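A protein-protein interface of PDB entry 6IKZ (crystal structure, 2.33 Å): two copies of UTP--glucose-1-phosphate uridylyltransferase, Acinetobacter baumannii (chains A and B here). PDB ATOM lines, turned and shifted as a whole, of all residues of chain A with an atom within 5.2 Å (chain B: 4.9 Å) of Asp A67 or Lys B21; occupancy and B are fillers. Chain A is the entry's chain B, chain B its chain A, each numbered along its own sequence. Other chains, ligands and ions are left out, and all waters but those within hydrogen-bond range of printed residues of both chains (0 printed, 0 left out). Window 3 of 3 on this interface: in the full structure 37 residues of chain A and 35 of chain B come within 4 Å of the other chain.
The side-chain amide oxygen of Asn A69 is in hydrogen-bond range of the backbone NH of Leu A72.
O of Tyr A65 lies within hydrogen-bond range of NZ of Lys B21 (2.6 Å).
The backbone carbonyl oxygen (O) of Asp A67 lies within hydrogen-bond range of the side-chain amino group (NZ) of Lys B21.
The side-chain amide nitrogen of Asn A69 is in hydrogen-bond range of the backbone carbonyl oxygen of Lys B21 (3.4 Å).
The side-chain amino group of Lys B21 sits at hydrogen-bond distance from the backbone carbonyl oxygen of Ile A88, 3.0 Å away.
N of Tyr A65 sits at hydrogen-bond distance from OG of Ser B22, at 3.1 Å.
O of Asn A64 touches CE of Lys B21, 3.7 Å away.
Asn A64 touches Ser B22 (C to OG, 3.4 Å).
CB of Pro B18 touches OH of Tyr A65 (3.5 Å).
Leu B17 touches Ile A88 (CG to CG2, 3.6 Å).
CG1 of Ile A91 touches NZ of Lys B21, at 3.97 Å.
Hydrophobic or aromatic side chains of chain A within 4 Å of the printed part of chain B: Tyr A65, Ile A88 and Ile A91.
Of the 7 printed residues of chain B, 4 touch a printed residue of chain A.
Printed residues of chain B that touch a printed residue of chain A: Leu B17, Pro B18, Lys B21 and Ser B22.
Along chain B the printed residues that touch a printed residue of chain A span positions 17 to 22.
Among the printed residues, no Asp or Glu carboxylate lies within 4 Å of a Lys or Arg side-chain nitrogen of the other chain.
No position is printed for both chains.
Of the 10 pairs that touch across the chains among the printed residues, none has its exchanged pair printed and touching as well.
Of the printed residues of chain B, Asn A69 touches Lys B21.
Leu A72 touches none of the printed residues of chain B.
Printed residues of chain B within 4 Å of Ile A91: Lys B21 (3.97 Å).
Lys B21 touches just these residues of chain A: Asn A64 (3.7 Å), Tyr A65 (2.6 Å), Asp A67 (2.6 Å), Asn A69 (3.4 Å), Ile A88 (3.0 Å) and Ile A91 (3.97 Å).
The nearest printed residue of chain B that does not touch Tyr A65 is Ala B19 (5.1 Å).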
ATOM      1  N   GLU A  63     -25.732   8.331 -22.684  1.00  0.00           N
ATOM      2  CA  GLU A  63     -24.558   9.119 -22.222  1.00  0.00           C
ATOM      3  C   GLU A  63     -24.885  10.605 -22.406  1.00  0.00           C
ATOM      4  O   GLU A  63     -24.803  11.345 -21.429  1.00  0.00           O
ATOM      5  CB  GLU A  63     -23.278   8.715 -22.949  1.00  0.00           C
ATOM      6  CG  GLU A  63     -22.828   7.300 -22.587  1.00  0.00           C
ATOM      7  CD  GLU A  63     -22.269   6.476 -23.746  1.00  0.00           C
ATOM      8  OE1 GLU A  63     -22.622   5.277 -23.841  1.00  0.00           O
ATOM      9  OE2 GLU A  63     -21.506   7.040 -24.580  1.00  0.00           O
ATOM     10  N   ASN A  64     -25.357  10.989 -23.587  1.00  0.00           N
ATOM     11  CA  ASN A  64     -25.741  12.381 -23.955  1.00  0.00           C
ATOM     12  C   ASN A  64     -26.655  13.027 -22.893  1.00  0.00           C
ATOM     13  O   ASN A  64     -26.459  14.223 -22.593  1.00  0.00           O
ATOM     14  CB  ASN A  64     -26.379  12.402 -25.352  1.00  0.00           C
ATOM     15  CG  ASN A  64     -25.360  12.128 -26.440  1.00  0.00           C
ATOM     16  OD1 ASN A  64     -24.146  12.264 -26.225  1.00  0.00           O
ATOM     17  ND2 ASN A  64     -25.840  11.736 -27.607  1.00  0.00           N
ATOM     18  N   TYR A  65     -27.668  12.304 -22.415  1.00  0.00           N
ATOM     19  CA  TYR A  65     -28.685  12.798 -21.457  1.00  0.00           C
ATOM     20  C   TYR A  65     -27.987  13.323 -20.192  1.00  0.00           C
ATOM     21  O   TYR A  65     -28.463  14.265 -19.612  1.00  0.00           O
ATOM     22  CB  TYR A  65     -29.644  11.661 -21.085  1.00  0.00           C
ATOM     23  CG  TYR A  65     -30.799  12.132 -20.259  1.00  0.00           C
ATOM     24  CD1 TYR A  65     -31.821  12.819 -20.856  1.00  0.00           C
ATOM     25  CD2 TYR A  65     -30.837  11.964 -18.895  1.00  0.00           C
ATOM     26  CE1 TYR A  65     -32.887  13.320 -20.134  1.00  0.00           C
ATOM     27  CE2 TYR A  65     -31.906  12.443 -18.148  1.00  0.00           C
ATOM     28  CZ  TYR A  65     -32.941  13.126 -18.772  1.00  0.00           C
ATOM     29  OH  TYR A  65     -34.018  13.648 -18.105  1.00  0.00           O
ATOM     30  N   PHE A  66     -26.871  12.740 -19.766  1.00  0.00           N
ATOM     31  CA  PHE A  66     -26.153  13.184 -18.545  1.00  0.00           C
ATOM     32  C   PHE A  66     -24.977  14.059 -18.962  1.00  0.00           C
ATOM     33  O   PHE A  66     -24.104  14.279 -18.142  1.00  0.00           O
ATOM     34  CB  PHE A  66     -25.759  11.982 -17.673  1.00  0.00           C
ATOM     35  CG  PHE A  66     -26.946  11.173 -17.226  1.00  0.00           C
ATOM     36  CD1 PHE A  66     -27.824  11.661 -16.285  1.00  0.00           C
ATOM     37  CD2 PHE A  66     -27.223   9.933 -17.781  1.00  0.00           C
ATOM     38  CE1 PHE A  66     -28.951  10.933 -15.902  1.00  0.00           C
ATOM     39  CE2 PHE A  66     -28.340   9.208 -17.388  1.00  0.00           C
ATOM     40  CZ  PHE A  66     -29.195   9.702 -16.435  1.00  0.00           C
ATOM     41  N   ASP A  67     -24.955  14.533 -20.201  1.00  0.00           N
ATOM     42  CA  ASP A  67     -23.893  15.440 -20.711  1.00  0.00           C
ATOM     43  C   ASP A  67     -24.600  16.747 -21.072  1.00  0.00           C
ATOM     44  O   ASP A  67     -25.858  16.808 -20.948  1.00  0.00           O
ATOM     45  CB  ASP A  67     -23.135  14.807 -21.878  1.00  0.00           C
ATOM     46  CG  ASP A  67     -21.823  15.490 -22.264  1.00  0.00           C
ATOM     47  OD1 ASP A  67     -21.350  16.351 -21.494  1.00  0.00           O
ATOM     48  OD2 ASP A  67     -21.281  15.179 -23.366  1.00  0.00           O
ATOM     49  N   ARG A  68     -23.853  17.756 -21.517  1.00  0.00           N
ATOM     50  CA  ARG A  68     -24.425  19.062 -21.878  1.00  0.00           C
ATOM     51  C   ARG A  68     -24.649  19.076 -23.384  1.00  0.00           C
ATOM     52  O   ARG A  68     -23.859  18.473 -24.095  1.00  0.00           O
ATOM     53  CB  ARG A  68     -23.549  20.154 -21.256  1.00  0.00           C
ATOM     54  CG  ARG A  68     -24.109  20.557 -19.895  1.00  0.00           C
ATOM     55  CD  ARG A  68     -23.195  20.836 -18.715  1.00  0.00           C
ATOM     56  NE  ARG A  68     -22.546  22.129 -18.820  1.00  0.00           N
ATOM     57  CZ  ARG A  68     -23.177  23.287 -18.928  1.00  0.00           C
ATOM     58  NH1 ARG A  68     -24.497  23.344 -18.949  1.00  0.00           N
ATOM     59  NH2 ARG A  68     -22.473  24.394 -19.042  1.00  0.00           N
ATOM     60  N   ASN A  69     -25.736  19.706 -23.818  1.00  0.00           N
ATOM     61  CA  ASN A  69     -26.142  19.807 -25.241  1.00  0.00           C
ATOM     62  C   ASN A  69     -25.947  21.268 -25.715  1.00  0.00           C
ATOM     63  O   ASN A  69     -26.875  22.090 -25.562  1.00  0.00           O
ATOM     64  CB  ASN A  69     -27.563  19.258 -25.393  1.00  0.00           C
ATOM     65  CG  ASN A  69     -28.068  19.299 -26.820  1.00  0.00           C
ATOM     66  OD1 ASN A  69     -27.539  20.036 -27.656  1.00  0.00           O
ATOM     67  ND2 ASN A  69     -29.133  18.562 -27.090  1.00  0.00           N
ATOM     68  N   LEU A  72     -28.799  23.078 -27.862  1.00  0.00           N
ATOM     69  CA  LEU A  72     -30.104  23.198 -27.156  1.00  0.00           C
ATOM     70  C   LEU A  72     -29.940  24.195 -26.009  1.00  0.00           C
ATOM     71  O   LEU A  72     -30.857  24.963 -25.761  1.00  0.00           O
ATOM     72  CB  LEU A  72     -30.571  21.826 -26.645  1.00  0.00           C
ATOM     73  CG  LEU A  72     -31.886  21.859 -25.876  1.00  0.00           C
ATOM     74  CD1 LEU A  72     -33.038  22.070 -26.826  1.00  0.00           C
ATOM     75  CD2 LEU A  72     -32.095  20.595 -25.059  1.00  0.00           C
ATOM     76  N   ILE A  88     -32.317  20.711 -17.884  1.00  0.00           N
ATOM     77  CA  ILE A  88     -31.370  19.984 -18.789  1.00  0.00           C
ATOM     78  C   ILE A  88     -29.915  20.133 -18.328  1.00  0.00           C
ATOM     79  O   ILE A  88     -29.102  19.373 -18.839  1.00  0.00           O
ATOM     80  CB  ILE A  88     -31.551  20.322 -20.299  1.00  0.00           C
ATOM     81  CG1 ILE A  88     -31.063  21.704 -20.763  1.00  0.00           C
ATOM     82  CG2 ILE A  88     -33.002  20.088 -20.690  1.00  0.00           C
ATOM     83  N   ILE A  91     -28.750  17.609 -13.925  1.00  0.00           N
ATOM     84  CA  ILE A  91     -29.461  16.296 -13.964  1.00  0.00           C
ATOM     85  C   ILE A  91     -28.972  15.514 -12.752  1.00  0.00           C
ATOM     86  O   ILE A  91     -29.790  14.952 -12.019  1.00  0.00           O
ATOM     87  CB  ILE A  91     -29.243  15.530 -15.283  1.00  0.00           C
ATOM     88  CG1 ILE A  91     -29.646  16.339 -16.523  1.00  0.00           C
ATOM     89  CG2 ILE A  91     -29.983  14.201 -15.223  1.00  0.00           C
ATOM     90  CD1 ILE A  91     -31.079  16.121 -16.997  1.00  0.00           C
ATOM     91  N   LEU B  17     -39.167  19.212 -22.625  1.00  0.00           N
ATOM     92  CA  LEU B  17     -37.892  18.862 -21.940  1.00  0.00           C
ATOM     93  C   LEU B  17     -38.229  18.358 -20.536  1.00  0.00           C
ATOM     94  O   LEU B  17     -39.265  18.722 -19.985  1.00  0.00           O
ATOM     95  CB  LEU B  17     -37.039  20.125 -21.850  1.00  0.00           C
ATOM     96  CG  LEU B  17     -35.899  20.305 -22.848  1.00  0.00           C
ATOM     97  CD1 LEU B  17     -36.128  19.610 -24.144  1.00  0.00           C
ATOM     98  CD2 LEU B  17     -35.661  21.770 -23.115  1.00  0.00           C
ATOM     99  N   PRO B  18     -37.384  17.529 -19.879  1.00  0.00           N
ATOM    100  CA  PRO B  18     -36.141  16.998 -20.463  1.00  0.00           C
ATOM    101  C   PRO B  18     -36.310  15.727 -21.328  1.00  0.00           C
ATOM    102  O   PRO B  18     -35.317  15.204 -21.864  1.00  0.00           O
ATOM    103  CB  PRO B  18     -35.300  16.668 -19.205  1.00  0.00           C
ATOM    104  CG  PRO B  18     -36.345  16.283 -18.166  1.00  0.00           C
ATOM    105  CD  PRO B  18     -37.581  17.107 -18.485  1.00  0.00           C
ATOM    106  N   ALA B  19     -37.551  15.242 -21.439  1.00  0.00           N
ATOM    107  CA  ALA B  19     -37.936  14.067 -22.247  1.00  0.00           C
ATOM    108  C   ALA B  19     -37.246  14.104 -23.613  1.00  0.00           C
ATOM    109  O   ALA B  19     -36.888  13.024 -24.097  1.00  0.00           O
ATOM    110  CB  ALA B  19     -39.442  14.023 -22.388  1.00  0.00           C
ATOM    111  N   SER B  20     -37.071  15.287 -24.213  1.00  0.00           N
ATOM    112  CA  SER B  20     -36.512  15.446 -25.576  1.00  0.00           C
ATOM    113  C   SER B  20     -35.141  16.101 -25.502  1.00  0.00           C
ATOM    114  O   SER B  20     -34.651  16.664 -26.518  1.00  0.00           O
ATOM    115  CB  SER B  20     -37.433  16.229 -26.429  1.00  0.00           C
ATOM    116  OG  SER B  20     -37.412  17.561 -25.995  1.00  0.00           O
ATOM    117  N   LYS B  21     -34.513  16.043 -24.336  1.00  0.00           N
ATOM    118  CA  LYS B  21     -33.123  16.551 -24.252  1.00  0.00           C
ATOM    119  C   LYS B  21     -32.303  15.833 -25.304  1.00  0.00           C
ATOM    120  O   LYS B  21     -31.633  16.516 -26.020  1.00  0.00           O
ATOM    121  CB  LYS B  21     -32.451  16.338 -22.894  1.00  0.00           C
ATOM    122  CG  LYS B  21     -31.034  16.907 -22.851  1.00  0.00           C
ATOM    123  CD  LYS B  21     -30.375  16.742 -21.513  1.00  0.00           C
ATOM    124  CE  LYS B  21     -28.873  16.829 -21.601  1.00  0.00           C
ATOM    125  NZ  LYS B  21     -28.315  16.812 -20.232  1.00  0.00           N
ATOM    126  N   SER B  22     -32.393  14.497 -25.339  1.00  0.00           N
ATOM    127  CA  SER B  22     -31.432  13.555 -25.976  1.00  0.00           C
ATOM    128  C   SER B  22     -32.087  12.578 -26.975  1.00  0.00           C
ATOM    129  O   SER B  22     -31.340  11.784 -27.522  1.00  0.00           O
ATOM    130  CB  SER B  22     -30.708  12.821 -24.907  1.00  0.00           C
ATOM    131  OG  SER B  22     -29.646  13.625 -24.423  1.00  0.00           O
ATOM    132  N   ILE B  23     -33.403  12.643 -27.213  1.00  0.00           N
ATOM    133  CA  ILE B  23     -34.132  11.908 -28.292  1.00  0.00           C
ATOM    134  C   ILE B  23     -35.108  12.893 -28.909  1.00  0.00           C
ATOM    135  O   ILE B  23     -35.616  13.754 -28.224  1.00  0.00           O
ATOM    136  CB  ILE B  23     -34.905  10.666 -27.773  1.00  0.00           C
ATOM    137  CG1 ILE B  23     -36.124  11.071 -26.950  1.00  0.00           C
ATOM    138  CG2 ILE B  23     -34.008   9.748 -26.980  1.00  0.00           C
ATOM    139  CD1 ILE B  23     -36.927   9.917 -26.408  1.00  0.00           C
